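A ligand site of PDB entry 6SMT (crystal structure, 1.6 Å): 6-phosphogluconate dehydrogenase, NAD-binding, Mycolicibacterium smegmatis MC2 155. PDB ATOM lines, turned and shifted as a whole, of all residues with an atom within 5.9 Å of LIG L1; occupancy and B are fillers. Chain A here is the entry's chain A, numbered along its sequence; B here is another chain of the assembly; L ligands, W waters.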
ATOM      1  N   GLY A  17      14.610 -22.438  -6.338  1.00  0.00           N
ATOM      2  CA  GLY A  17      13.248 -22.090  -5.989  1.00  0.00           C
ATOM      3  C   GLY A  17      12.648 -21.188  -7.020  1.00  0.00           C
ATOM      4  O   GLY A  17      13.085 -20.005  -7.121  1.00  0.00           O
ATOM      5  N   LEU A  18      11.741 -21.710  -7.858  1.00  0.00           N
ATOM      6  CA  LEU A  18      11.186 -20.984  -9.038  1.00  0.00           C
ATOM      7  C   LEU A  18       9.670 -20.898  -8.969  1.00  0.00           C
ATOM      8  O   LEU A  18       8.963 -20.998 -10.006  1.00  0.00           O
ATOM      9  CB  LEU A  18      11.662 -21.679 -10.293  1.00  0.00           C
ATOM     10  CG  LEU A  18      13.175 -21.808 -10.446  1.00  0.00           C
ATOM     11  CD1 LEU A  18      13.514 -22.505 -11.770  1.00  0.00           C
ATOM     12  CD2 LEU A  18      13.845 -20.436 -10.377  1.00  0.00           C
ATOM     13  N   GLY A  19       9.156 -20.635  -7.793  1.00  0.00           N
ATOM     14  CA  GLY A  19       7.837 -20.107  -7.621  1.00  0.00           C
ATOM     15  C   GLY A  19       7.764 -18.696  -8.128  1.00  0.00           C
ATOM     16  O   GLY A  19       8.703 -18.167  -8.691  1.00  0.00           O
ATOM     17  N   PRO A  20       6.657 -17.985  -7.893  1.00  0.00           N
ATOM     18  CA  PRO A  20       6.516 -16.640  -8.420  1.00  0.00           C
ATOM     19  C   PRO A  20       7.661 -15.691  -8.075  1.00  0.00           C
ATOM     20  O   PRO A  20       8.138 -14.913  -8.891  1.00  0.00           O
ATOM     21  CB  PRO A  20       5.186 -16.154  -7.944  1.00  0.00           C
ATOM     22  CG  PRO A  20       4.517 -17.380  -7.469  1.00  0.00           C
ATOM     23  CD  PRO A  20       5.467 -18.499  -7.248  1.00  0.00           C
ATOM     24  N   MET A  21       8.103 -15.700  -6.810  1.00  0.00           N
ATOM     25  CA  MET A  21       9.159 -14.822  -6.392  1.00  0.00           C
ATOM     26  C   MET A  21      10.483 -15.292  -6.989  1.00  0.00           C
ATOM     27  O   MET A  21      11.300 -14.420  -7.395  1.00  0.00           O
ATOM     28  CB  MET A  21       9.233 -14.694  -4.880  1.00  0.00           C
ATOM     29  CG  MET A  21      10.306 -13.765  -4.394  1.00  0.00           C
ATOM     30  SD  MET A  21      10.293 -12.070  -5.054  1.00  0.00           S
ATOM     31  CE  MET A  21       9.005 -11.402  -4.082  1.00  0.00           C
ATOM     32  N   GLY A  22      10.817 -16.563  -7.045  1.00  0.00           N
ATOM     33  CA  GLY A  22      12.074 -16.994  -7.630  1.00  0.00           C
ATOM     34  C   GLY A  22      12.133 -16.699  -9.108  1.00  0.00           C
ATOM     35  O   GLY A  22      13.213 -16.368  -9.602  1.00  0.00           O
ATOM     36  N   TRP A  39      17.369 -23.767 -10.584  1.00  0.00           N
ATOM     37  CA  TRP A  39      16.943 -25.114 -10.193  1.00  0.00           C
ATOM     38  C   TRP A  39      15.619 -24.967  -9.445  1.00  0.00           C
ATOM     39  O   TRP A  39      15.444 -24.071  -8.649  1.00  0.00           O
ATOM     40  CB  TRP A  39      17.977 -25.818  -9.285  1.00  0.00           C
ATOM     41  CG  TRP A  39      17.546 -27.134  -8.817  1.00  0.00           C
ATOM     42  CD1 TRP A  39      17.745 -28.353  -9.396  1.00  0.00           C
ATOM     43  CD2 TRP A  39      16.781 -27.385  -7.618  1.00  0.00           C
ATOM     44  NE1 TRP A  39      17.191 -29.353  -8.692  1.00  0.00           N
ATOM     45  CE2 TRP A  39      16.562 -28.789  -7.569  1.00  0.00           C
ATOM     46  CE3 TRP A  39      16.240 -26.583  -6.608  1.00  0.00           C
ATOM     47  CZ2 TRP A  39      15.850 -29.385  -6.537  1.00  0.00           C
ATOM     48  CZ3 TRP A  39      15.530 -27.214  -5.584  1.00  0.00           C
ATOM     49  CH2 TRP A  39      15.328 -28.568  -5.566  1.00  0.00           C
ATOM     50  N   ASN A  40      14.736 -25.903  -9.684  1.00  0.00           N
ATOM     51  CA  ASN A  40      13.509 -26.097  -8.915  1.00  0.00           C
ATOM     52  C   ASN A  40      13.243 -27.560  -8.698  1.00  0.00           C
ATOM     53  O   ASN A  40      13.434 -28.393  -9.605  1.00  0.00           O
ATOM     54  CB  ASN A  40      12.342 -25.388  -9.586  1.00  0.00           C
ATOM     55  CG  ASN A  40      11.102 -25.267  -8.754  1.00  0.00           C
ATOM     56  OD1 ASN A  40      11.161 -24.570  -7.730  1.00  0.00           O
ATOM     57  ND2 ASN A  40       9.991 -25.816  -9.151  1.00  0.00           N
ATOM     58  N   ARG A  41      12.584 -27.895  -7.599  1.00  0.00           N
ATOM     59  CA  ARG A  41      12.184 -29.292  -7.315  1.00  0.00           C
ATOM     60  C   ARG A  41      11.280 -29.835  -8.455  1.00  0.00           C
ATOM     61  O   ARG A  41      11.577 -30.943  -8.964  1.00  0.00           O
ATOM     62  CB  ARG A  41      11.447 -29.306  -5.972  1.00  0.00           C
ATOM     63  CG  ARG A  41      10.687 -30.581  -5.730  1.00  0.00           C
ATOM     64  CD  ARG A  41       9.937 -30.576  -4.432  1.00  0.00           C
ATOM     65  NE  ARG A  41       8.907 -29.644  -4.363  1.00  0.00           N
ATOM     66  CZ  ARG A  41       8.071 -29.487  -3.343  1.00  0.00           C
ATOM     67  NH1 ARG A  41       8.179 -30.315  -2.289  1.00  0.00           N
ATOM     68  NH2 ARG A  41       7.137 -28.615  -3.406  1.00  0.00           N
ATOM     69  N   THR A  42      10.306 -29.064  -8.858  1.00  0.00           N
ATOM     70  CA  THR A  42       9.514 -29.346 -10.056  1.00  0.00           C
ATOM     71  C   THR A  42      10.269 -28.762 -11.243  1.00  0.00           C
ATOM     72  O   THR A  42      10.240 -27.543 -11.490  1.00  0.00           O
ATOM     73  CB  THR A  42       8.107 -28.835  -9.871  1.00  0.00           C
ATOM     74  OG1 THR A  42       7.473 -29.324  -8.712  1.00  0.00           O
ATOM     75  CG2 THR A  42       7.283 -29.256 -11.080  1.00  0.00           C
ATOM     76  N   LYS A  45       9.440 -25.915 -14.160  1.00  0.00           N
ATOM     77  CA  LYS A  45       9.299 -24.478 -13.888  1.00  0.00           C
ATOM     78  C   LYS A  45      10.506 -23.695 -14.351  1.00  0.00           C
ATOM     79  O   LYS A  45      10.354 -22.468 -14.406  1.00  0.00           O
ATOM     80  CB  LYS A  45       9.003 -24.258 -12.391  1.00  0.00           C
ATOM     81  CG  LYS A  45       7.740 -24.919 -11.905  1.00  0.00           C
ATOM     82  CD  LYS A  45       7.148 -24.376 -10.620  1.00  0.00           C
ATOM     83  CE  LYS A  45       5.947 -25.164 -10.198  1.00  0.00           C
ATOM     84  NZ  LYS A  45       5.524 -24.815  -8.814  1.00  0.00           N
ATOM     85  N   ASN A  73      15.043 -19.435  -2.517  1.00  0.00           N
ATOM     86  CA  ASN A  73      13.767 -18.699  -2.404  1.00  0.00           C
ATOM     87  C   ASN A  73      12.665 -19.711  -2.502  1.00  0.00           C
ATOM     88  O   ASN A  73      12.102 -19.927  -3.609  1.00  0.00           O
ATOM     89  CB  ASN A  73      13.717 -17.602  -3.495  1.00  0.00           C
ATOM     90  CG  ASN A  73      12.453 -16.758  -3.413  1.00  0.00           C
ATOM     91  OD1 ASN A  73      11.662 -16.767  -4.360  1.00  0.00           O
ATOM     92  ND2 ASN A  73      12.274 -16.062  -2.296  1.00  0.00           N
ATOM     93  N   VAL A  74      12.334 -20.305  -1.389  1.00  0.00           N
ATOM     94  CA  VAL A  74      11.330 -21.373  -1.278  1.00  0.00           C
ATOM     95  C   VAL A  74      10.415 -21.103  -0.090  1.00  0.00           C
ATOM     96  O   VAL A  74      10.577 -20.119   0.611  1.00  0.00           O
ATOM     97  CB  VAL A  74      11.972 -22.767  -1.240  1.00  0.00           C
ATOM     98  CG1 VAL A  74      12.699 -23.104  -2.539  1.00  0.00           C
ATOM     99  CG2 VAL A  74      12.938 -22.813  -0.052  1.00  0.00           C
ATOM    100  N   VAL A  75       9.450 -21.982   0.128  1.00  0.00           N
ATOM    101  CA  VAL A  75       8.353 -21.643   1.086  1.00  0.00           C
ATOM    102  C   VAL A  75       8.908 -21.426   2.482  1.00  0.00           C
ATOM    103  O   VAL A  75       8.369 -20.493   3.148  1.00  0.00           O
ATOM    104  CB  VAL A  75       7.286 -22.729   1.013  1.00  0.00           C
ATOM    105  CG1 VAL A  75       7.761 -24.081   1.485  1.00  0.00           C
ATOM    106  CG2 VAL A  75       6.059 -22.279   1.810  1.00  0.00           C
ATOM    107  N   ASP A  76       9.875 -22.195   2.960  1.00  0.00           N
ATOM    108  CA  ASP A  76      10.290 -22.049   4.363  1.00  0.00           C
ATOM    109  C   ASP A  76      11.635 -22.731   4.529  1.00  0.00           C
ATOM    110  O   ASP A  76      12.255 -23.205   3.545  1.00  0.00           O
ATOM    111  CB  ASP A  76       9.260 -22.704   5.272  1.00  0.00           C
ATOM    112  CG  ASP A  76       9.113 -24.181   5.087  1.00  0.00           C
ATOM    113  OD1 ASP A  76       9.829 -24.934   4.448  1.00  0.00           O
ATOM    114  OD2 ASP A  76       7.978 -24.725   5.524  1.00  0.00           O
ATOM    115  N   ASP A  78      12.399 -25.434   6.288  1.00  0.00           N
ATOM    116  CA  ASP A  78      12.427 -26.888   6.044  1.00  0.00           C
ATOM    117  C   ASP A  78      12.803 -27.207   4.579  1.00  0.00           C
ATOM    118  O   ASP A  78      13.660 -28.067   4.333  1.00  0.00           O
ATOM    119  CB  ASP A  78      11.094 -27.516   6.413  1.00  0.00           C
ATOM    120  CG  ASP A  78      10.862 -27.700   7.867  1.00  0.00           C
ATOM    121  OD1 ASP A  78      11.806 -27.562   8.685  1.00  0.00           O
ATOM    122  OD2 ASP A  78       9.640 -27.978   8.225  1.00  0.00           O
ATOM    123  N   ALA A  79      12.292 -26.388   3.650  1.00  0.00           N
ATOM    124  CA  ALA A  79      12.629 -26.547   2.241  1.00  0.00           C
ATOM    125  C   ALA A  79      14.064 -26.124   1.990  1.00  0.00           C
ATOM    126  O   ALA A  79      14.813 -26.827   1.315  1.00  0.00           O
ATOM    127  CB  ALA A  79      11.630 -25.841   1.386  1.00  0.00           C
ATOM    128  N   ALA A  82      16.370 -28.822   3.381  1.00  0.00           N
ATOM    129  CA  ALA A  82      16.307 -30.028   2.535  1.00  0.00           C
ATOM    130  C   ALA A  82      17.124 -29.855   1.276  1.00  0.00           C
ATOM    131  O   ALA A  82      17.865 -30.737   0.832  1.00  0.00           O
ATOM    132  CB  ALA A  82      14.943 -30.370   2.199  1.00  0.00           C
ATOM    133  N   ILE A  83      17.074 -28.679   0.672  1.00  0.00           N
ATOM    134  CA  ILE A  83      17.869 -28.359  -0.538  1.00  0.00           C
ATOM    135  C   ILE A  83      19.337 -28.389  -0.159  1.00  0.00           C
ATOM    136  O   ILE A  83      20.166 -28.956  -0.902  1.00  0.00           O
ATOM    137  CB  ILE A  83      17.417 -27.023  -1.092  1.00  0.00           C
ATOM    138  CG1 ILE A  83      16.001 -27.161  -1.660  1.00  0.00           C
ATOM    139  CG2 ILE A  83      18.417 -26.467  -2.090  1.00  0.00           C
ATOM    140  CD1 ILE A  83      15.348 -25.795  -1.983  1.00  0.00           C
ATOM    141  N   LEU A  99      16.523 -16.577   1.226  1.00  0.00           N
ATOM    142  CA  LEU A  99      15.461 -15.592   0.984  1.00  0.00           C
ATOM    143  C   LEU A  99      14.142 -16.340   1.138  1.00  0.00           C
ATOM    144  O   LEU A  99      13.212 -16.149   0.366  1.00  0.00           O
ATOM    145  CB  LEU A  99      15.582 -15.022  -0.419  1.00  0.00           C
ATOM    146  CG  LEU A  99      16.841 -14.197  -0.616  1.00  0.00           C
ATOM    147  CD1 LEU A  99      16.997 -13.884  -2.116  1.00  0.00           C
ATOM    148  CD2 LEU A  99      16.838 -12.949   0.207  1.00  0.00           C
ATOM    149  N   SER A 100      13.989 -17.102   2.161  1.00  0.00           N
ATOM    150  CA  SER A 100      12.800 -17.949   2.412  1.00  0.00           C
ATOM    151  C   SER A 100      12.260 -17.584   3.768  1.00  0.00           C
ATOM    152  O   SER A 100      12.980 -17.735   4.816  1.00  0.00           O
ATOM    153  CB  SER A 100      13.142 -19.388   2.322  1.00  0.00           C
ATOM    154  OG  SER A 100      13.718 -19.698   1.059  1.00  0.00           O
ATOM    155  N   SER A 101      11.071 -17.051   3.872  1.00  0.00           N
ATOM    156  CA  SER A 101      10.522 -16.493   5.119  1.00  0.00           C
ATOM    157  C   SER A 101      10.380 -17.522   6.205  1.00  0.00           C
ATOM    158  O   SER A 101       9.667 -18.507   6.034  1.00  0.00           O
ATOM    159  CB  SER A 101       9.250 -15.726   4.806  1.00  0.00           C
ATOM    160  OG  SER A 101       8.767 -15.119   6.008  1.00  0.00           O
ATOM    161  N   ILE A 126      12.566 -10.512   1.858  1.00  0.00           N
ATOM    162  CA  ILE A 126      12.005  -9.693   0.765  1.00  0.00           C
ATOM    163  C   ILE A 126      10.692  -9.128   1.311  1.00  0.00           C
ATOM    164  O   ILE A 126       9.778  -9.878   1.679  1.00  0.00           O
ATOM    165  CB  ILE A 126      11.811 -10.455  -0.537  1.00  0.00           C
ATOM    166  CG1 ILE A 126      13.111 -11.103  -0.997  1.00  0.00           C
ATOM    167  CG2 ILE A 126      11.160  -9.592  -1.574  1.00  0.00           C
ATOM    168  CD1 ILE A 126      12.888 -12.285  -1.976  1.00  0.00           C
ATOM    169  N   MET A 127      10.573  -7.787   1.311  1.00  0.00           N
ATOM    170  CA  MET A 127       9.401  -7.162   2.013  1.00  0.00           C
ATOM    171  C   MET A 127       8.418  -6.547   1.025  1.00  0.00           C
ATOM    172  O   MET A 127       7.511  -5.803   1.434  1.00  0.00           O
ATOM    173  CB  MET A 127       9.921  -6.134   3.012  1.00  0.00           C
ATOM    174  CG  MET A 127      10.928  -6.610   4.023  1.00  0.00           C
ATOM    175  SD  MET A 127      10.464  -8.142   4.845  1.00  0.00           S
ATOM    176  CE  MET A 127       8.806  -7.756   5.385  1.00  0.00           C
ATOM    177  N   THR A 128       8.525  -6.839  -0.236  1.00  0.00           N
ATOM    178  CA  THR A 128       7.697  -6.219  -1.309  1.00  0.00           C
ATOM    179  C   THR A 128       7.263  -7.284  -2.260  1.00  0.00           C
ATOM    180  O   THR A 128       7.930  -8.330  -2.435  1.00  0.00           O
ATOM    181  CB  THR A 128       8.426  -5.068  -1.971  1.00  0.00           C
ATOM    182  OG1 THR A 128       9.743  -5.524  -2.359  1.00  0.00           O
ATOM    183  CG2 THR A 128       8.638  -3.918  -1.047  1.00  0.00           C
ATOM    184  N   PRO A 129       6.189  -7.079  -3.009  1.00  0.00           N
ATOM    185  CA  PRO A 129       5.644  -8.093  -3.892  1.00  0.00           C
ATOM    186  C   PRO A 129       6.425  -8.284  -5.190  1.00  0.00           C
ATOM    187  O   PRO A 129       7.348  -7.507  -5.534  1.00  0.00           O
ATOM    188  CB  PRO A 129       4.208  -7.653  -4.172  1.00  0.00           C
ATOM    189  CG  PRO A 129       4.233  -6.247  -3.905  1.00  0.00           C
ATOM    190  CD  PRO A 129       5.263  -5.924  -2.861  1.00  0.00           C
ATOM    191  N   ILE A 130       6.046  -9.301  -5.962  1.00  0.00           N
ATOM    192  CA  ILE A 130       6.884  -9.688  -7.132  1.00  0.00           C
ATOM    193  C   ILE A 130       7.022  -8.564  -8.166  1.00  0.00           C
ATOM    194  O   ILE A 130       8.104  -8.486  -8.782  1.00  0.00           O
ATOM    195  CB  ILE A 130       6.460 -10.995  -7.787  1.00  0.00           C
ATOM    196  CG1 ILE A 130       5.097 -10.896  -8.423  1.00  0.00           C
ATOM    197  CG2 ILE A 130       6.532 -12.187  -6.870  1.00  0.00           C
ATOM    198  CD1 ILE A 130       4.756 -12.063  -9.314  1.00  0.00           C
ATOM    199  N   LEU A 180       5.601  -8.785   8.705  1.00  0.00           N
ATOM    200  CA  LEU A 180       4.580  -9.687   8.108  1.00  0.00           C
ATOM    201  C   LEU A 180       3.407  -9.800   9.083  1.00  0.00           C
ATOM    202  O   LEU A 180       2.294 -10.014   8.570  1.00  0.00           O
ATOM    203  CB  LEU A 180       5.197 -11.068   7.885  1.00  0.00           C
ATOM    204  CG  LEU A 180       6.218 -11.099   6.742  1.00  0.00           C
ATOM    205  CD1 LEU A 180       6.834 -12.520   6.695  1.00  0.00           C
ATOM    206  CD2 LEU A 180       5.662 -10.724   5.416  1.00  0.00           C
ATOM    207  N   SER B 238       0.216 -14.798  -7.513  1.00  0.00           N
ATOM    208  CA  SER B 238       1.622 -14.368  -7.267  1.00  0.00           C
ATOM    209  C   SER B 238       1.979 -14.607  -5.796  1.00  0.00           C
ATOM    210  O   SER B 238       3.179 -14.426  -5.467  1.00  0.00           O
ATOM    211  CB  SER B 238       1.870 -12.930  -7.596  1.00  0.00           C
ATOM    212  OG  SER B 238       1.098 -12.069  -6.738  1.00  0.00           O
ATOM    213  N   ALA B 239       1.020 -14.857  -4.936  1.00  0.00           N
ATOM    214  CA  ALA B 239       1.303 -15.209  -3.517  1.00  0.00           C
ATOM    215  C   ALA B 239       0.173 -16.186  -3.098  1.00  0.00           C
ATOM    216  O   ALA B 239      -0.998 -15.754  -2.983  1.00  0.00           O
ATOM    217  CB  ALA B 239       1.328 -13.996  -2.637  1.00  0.00           C
ATOM    218  N   SER B 240       0.547 -17.408  -2.870  1.00  0.00           N
ATOM    219  CA  SER B 240      -0.460 -18.481  -2.690  1.00  0.00           C
ATOM    220  C   SER B 240      -0.894 -18.612  -1.230  1.00  0.00           C
ATOM    221  O   SER B 240      -0.161 -18.305  -0.231  1.00  0.00           O
ATOM    222  CB  SER B 240      -0.010 -19.770  -3.176  1.00  0.00           C
ATOM    223  OG  SER B 240       0.978 -20.349  -2.290  1.00  0.00           O
ATOM    224  N   SER B 242      -1.175 -21.530   0.257  1.00  0.00           N
ATOM    225  CA  SER B 242      -0.267 -22.530   0.844  1.00  0.00           C
ATOM    226  C   SER B 242       0.978 -21.816   1.421  1.00  0.00           C
ATOM    227  O   SER B 242       1.448 -22.154   2.502  1.00  0.00           O
ATOM    228  CB  SER B 242       0.086 -23.581  -0.122  1.00  0.00           C
ATOM    229  OG  SER B 242       0.762 -23.080  -1.284  1.00  0.00           O
ATOM    230  N   SER B 243       1.471 -20.793   0.732  1.00  0.00           N
ATOM    231  CA  SER B 243       2.641 -20.077   1.242  1.00  0.00           C
ATOM    232  C   SER B 243       2.327 -19.380   2.550  1.00  0.00           C
ATOM    233  O   SER B 243       3.120 -19.407   3.507  1.00  0.00           O
ATOM    234  CB  SER B 243       3.165 -19.124   0.128  1.00  0.00           C
ATOM    235  OG  SER B 243       4.413 -18.548   0.550  1.00  0.00           O
ATOM    236  N   SER B 247       3.757 -19.348   6.431  1.00  0.00           N
ATOM    237  CA  SER B 247       4.224 -18.105   7.055  1.00  0.00           C
ATOM    238  C   SER B 247       3.539 -17.793   8.377  1.00  0.00           C
ATOM    239  O   SER B 247       4.183 -17.453   9.381  1.00  0.00           O
ATOM    240  CB  SER B 247       4.083 -16.953   6.057  1.00  0.00           C
ATOM    241  OG  SER B 247       4.690 -15.794   6.652  1.00  0.00           O
HETATM  242  P1  LIG L   1       6.140 -20.263  -2.090  1.00  0.00           P
HETATM  243  O1  LIG L   1       6.357 -19.660  -0.775  1.00  0.00           O
HETATM  244  O2  LIG L   1       4.796 -20.781  -2.461  1.00  0.00           O
HETATM  245  O3  LIG L   1       7.177 -21.430  -2.251  1.00  0.00           O
HETATM  246  C1  LIG L   1       7.134 -22.271  -3.464  1.00  0.00           C
HETATM  247  C2  LIG L   1       8.529 -22.698  -3.817  1.00  0.00           C
HETATM  248  O4  LIG L   1       9.095 -23.509  -2.746  1.00  0.00           O
HETATM  249  C3  LIG L   1       8.552 -23.580  -5.088  1.00  0.00           C
HETATM  250  O5  LIG L   1       9.784 -23.365  -5.763  1.00  0.00           O
HETATM  251  C4  LIG L   1       8.490 -24.978  -4.470  1.00  0.00           C
HETATM  252  O6  LIG L   1       8.931 -26.022  -5.287  1.00  0.00           O
HETATM  253  C5  LIG L   1       9.453 -24.744  -3.320  1.00  0.00           C
HETATM  254  N1  LIG L   1       9.432 -25.768  -2.291  1.00  0.00           N
HETATM  255  C6  LIG L   1       8.409 -26.039  -1.401  1.00  0.00           C
HETATM  256  N2  LIG L   1       8.688 -27.069  -0.614  1.00  0.00           N
HETATM  257  C7  LIG L   1       9.891 -27.544  -1.055  1.00  0.00           C
HETATM  258  C8  LIG L   1      10.746 -28.625  -0.690  1.00  0.00           C
HETATM  259  N3  LIG L   1      10.472 -29.430   0.336  1.00  0.00           N
HETATM  260  N4  LIG L   1      11.871 -28.806  -1.398  1.00  0.00           N
HETATM  261  C9  LIG L   1      12.158 -27.983  -2.405  1.00  0.00           C
HETATM  262  N5  LIG L   1      11.484 -26.908  -2.808  1.00  0.00           N
HETATM  263  C10 LIG L   1      10.358 -26.754  -2.120  1.00  0.00           C
HETATM  264  O7  LIG L   1       6.623 -19.335  -3.319  1.00  0.00           O
HETATM  265  P2  LIG L   1       6.918 -17.800  -3.563  1.00  0.00           P
HETATM  266  O8  LIG L   1       7.727 -17.741  -4.796  1.00  0.00           O
HETATM  267  O9  LIG L   1       5.623 -17.094  -3.511  1.00  0.00           O
HETATM  268  O10 LIG L   1       7.699 -17.316  -2.306  1.00  0.00           O
HETATM  269  C11 LIG L   1       9.041 -17.822  -2.012  1.00  0.00           C
HETATM  270  C12 LIG L   1       9.504 -17.165  -0.746  1.00  0.00           C
HETATM  271  O11 LIG L   1       9.568 -15.725  -0.967  1.00  0.00           O
HETATM  272  C13 LIG L   1       8.606 -17.373   0.467  1.00  0.00           C
HETATM  273  O12 LIG L   1       9.373 -17.684   1.628  1.00  0.00           O
HETATM  274  C14 LIG L   1       7.817 -16.087   0.555  1.00  0.00           C
HETATM  275  O13 LIG L   1       7.387 -15.747   1.879  1.00  0.00           O
HETATM  276  C15 LIG L   1       8.859 -15.077   0.042  1.00  0.00           C
HETATM  277  N6  LIG L   1       8.211 -13.874  -0.507  1.00  0.00           N
HETATM  278  C16 LIG L   1       7.278 -13.970  -1.513  1.00  0.00           C
HETATM  279  C17 LIG L   1       6.638 -12.870  -2.006  1.00  0.00           C
HETATM  280  C18 LIG L   1       5.623 -12.988  -3.040  1.00  0.00           C
HETATM  281  O14 LIG L   1       5.053 -11.910  -3.380  1.00  0.00           O
HETATM  282  N7  LIG L   1       5.294 -14.111  -3.661  1.00  0.00           N
HETATM  283  C19 LIG L   1       6.918 -11.551  -1.408  1.00  0.00           C
HETATM  284  C20 LIG L   1       7.947 -11.528  -0.438  1.00  0.00           C
HETATM  285  C21 LIG L   1       8.549 -12.634  -0.029  1.00  0.00           C
HETATM  286  P3  LIG L   1       7.852 -26.638  -6.359  1.00  0.00           P
HETATM  287  O15 LIG L   1       7.729 -25.641  -7.500  1.00  0.00           O
HETATM  288  O16 LIG L   1       8.474 -27.922  -6.755  1.00  0.00           O
HETATM  289  O17 LIG L   1       6.524 -26.832  -5.623  1.00  0.00           O
HETATM  290  C1  LG2 L   2       4.055 -10.924   1.822  1.00  0.00           C
HETATM  291  C2  LG2 L   2       5.191  -8.790   1.102  1.00  0.00           C
HETATM  292  C3  LG2 L   2       5.525  -8.343   2.521  1.00  0.00           C
HETATM  293  C4  LG2 L   2       2.179 -10.513  -0.583  1.00  0.00           C
HETATM  294  C5  LG2 L   2       3.963  -9.645   0.991  1.00  0.00           C
HETATM  295  O1  LG2 L   2       4.803 -11.989   1.261  1.00  0.00           O
HETATM  296  C6  LG2 L   2       3.540  -9.880  -0.447  1.00  0.00           C
HETATM  297  C7  LG2 L   2       1.512 -10.229  -1.846  1.00  0.00           C
HETATM  298  C8  LG2 L   2       0.044 -10.626  -1.826  1.00  0.00           C
HETATM  299  O   HOH W   1       3.513 -10.780  -5.180  1.00  0.00           O
HETATM  300  O   HOH W   2       5.258 -24.978  -1.903  1.00  0.00           O
HETATM  301  O   HOH W   3       4.630 -28.588  -6.117  1.00  0.00           O
HETATM  302  O   HOH W   4       4.471 -16.241  -1.066  1.00  0.00           O
HETATM  303  O   HOH W   5      11.570 -31.609   1.869  1.00  0.00           O
HETATM  304  O   HOH W   6       3.196 -18.398  -3.859  1.00  0.00           O
HETATM  305  O   HOH W   7       6.802 -13.245   2.976  1.00  0.00           O
HETATM  306  O   HOH W   8       4.832 -24.769  -5.176  1.00  0.00           O
HETATM  307  O   HOH W   9       7.207 -27.896   1.444  1.00  0.00           O
HETATM  308  O   HOH W  10      10.038 -19.106  -5.548  1.00  0.00           O
HETATM  309  O   HOH W  11      12.342 -25.951  -5.419  1.00  0.00           O
HETATM  310  O   HOH W  12       5.693 -17.583   2.837  1.00  0.00           O
HETATM  311  O   HOH W  13      10.855 -29.976   3.485  1.00  0.00           O
HETATM  312  O   HOH W  14       3.559 -22.964  -1.175  1.00  0.00           O
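The backbone carbonyl oxygen (O) of Trp 39 sits at hydrogen-bond distance from the backbone NH (N) of Gly 17 (3.0 Å).
OG of Ser 240 of chain B lies within hydrogen-bond range of OG of Ser 242 of chain B (2.9 Å).
N of Val 74 is in hydrogen-bond range of OG of Ser 100 (2.9 Å).
ND2 of Asn 40 lies within hydrogen-bond range of O of Thr 42 (2.9 Å).
N of Leu 18 sits at hydrogen-bond distance from OD1 of Asn 40.
The side-chain carboxylate of Asp 76 is in hydrogen-bond range of the backbone NH of Ala 79, at 3.0 Å.
ND2 of Asn 73 sits at hydrogen-bond distance from O of Leu 99.
The side-chain amide oxygen (OD1) of Asn 73 sits at hydrogen-bond distance from the backbone NH (N) of Gly 22 (2.8 Å).
Water W12 lies within hydrogen-bond range of O13 of LIG L1 and OG of Ser 243 of chain B.
Water W6 bridges O9 of LIG L1 (2.8 Å) and N of Ser 240 of chain B (3.0 Å).
Water W10 lies within hydrogen-bond range of an oxygen (O8) of LIG L1, the backbone NH (N) of Gly 19, the backbone carbonyl oxygen (O) of Asn 73 and the backbone NH (N) of Gly 22.
Water W7 lies within hydrogen-bond range of an oxygen (O13) of LIG L1 and an oxygen (O1) of LG2 L2.
Water W14 lies within hydrogen-bond range of OG of Ser 242 of chain B and O2 of LIG L1.
Water W13 bridges a nitrogen (N3) of LIG L1 and the backbone carbonyl oxygen (O) of Asp 78.
An oxygen (O8) of LIG L1 sits at hydrogen-bond distance from the backbone NH of Met 21 (2.9 Å).
The backbone carbonyl oxygen (O) of Val 74 sits at hydrogen-bond distance from an oxygen (O12) of LIG L1.
The backbone carbonyl oxygen (O) of Val 75 sits at hydrogen-bond distance from an oxygen (O12) of LIG L1 (3.3 Å).
OD1 of Asn 40 lies within hydrogen-bond range of O5 of LIG L1 (2.7 Å).
N of Val 75 is in hydrogen-bond range of O4 of LIG L1 (3.3 Å).
The side-chain hydroxyl (OG) of Ser 243 of chain B lies within hydrogen-bond range of an oxygen (O1) of LIG L1 (2.6 Å).
An oxygen (O17) of LIG L1 lies within salt-bridge range of the guanidinium group (NH2) of Arg 41 (2.9 Å).
N of Gly 19 is in hydrogen-bond range of O5 of LIG L1 (3.5 Å).
OG1 of Thr 42 sits at hydrogen-bond distance from O16 of LIG L1.
The backbone NH (N) of Ser 101 is in hydrogen-bond range of an oxygen (O12) of LIG L1 (2.9 Å).
N of Thr 42 lies within hydrogen-bond range of O16 of LIG L1, 3.0 Å away.
The backbone NH (N) of Leu 18 lies within hydrogen-bond range of an oxygen (O5) of LIG L1, 3.3 Å away.
The side-chain amino group (NZ) of Lys 45 is in salt-bridge range of an oxygen (O15) of LIG L1 (2.7 Å).
The side-chain amide nitrogen (ND2) of Asn 73 is in hydrogen-bond range of an oxygen (O11) of LIG L1 (3.0 Å).
O of Ser 238 of chain B is in hydrogen-bond range of N7 of LIG L1 (2.8 Å).
N of Pro 20 sits close to O8 of LIG L1, at 3.3 Å.
CA of Gly 17 touches O5 of LIG L1, at 3.7 Å.
Gly 22 touches LIG L1 (N to O8, 3.999 Å).
Ala 79 touches LIG L1.
CD1 of Ile 83 touches C9 of LIG L1 (3.9 Å).
O of Leu 99 touches O11 of LIG L1, at 3.9 Å.
Ser 100 touches LIG L1.
Ile 126 touches LIG L1 (O to C20, 3.2 Å).
Thr 128 touches LIG L1 (O to C19, 3.5 Å).
Pro 129 touches LIG L1.
Ile 130 touches LIG L1.
Ser 240 of chain B touches LIG L1 (OG to O2, 3.8 Å).
Hydrophobic or aromatic side chains within 4 Å of LIG L1: Pro 20, Met 21, Val 74, Val 75, Ala 79, Ile 83, Ile 126 and Ile 130.
Within 4 Å of LIG L1: Gly 17, Leu 18, Gly 19, Pro 20, Met 21, Gly 22, Asn 40, Arg 41, Thr 42, Lys 45, Asn 73, Val 74, Val 75, Ala 79, Ile 83, Leu 99, Ser 100, Ser 101, Ile 126, Thr 128, Pro 129, Ile 130, Ser 238 of chain B, Ser 240 of chain B and Ser 243 of chain B.
The nearest printed residue that does not touch LIG L1 is Ala 239 of chain B (4.1 Å).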
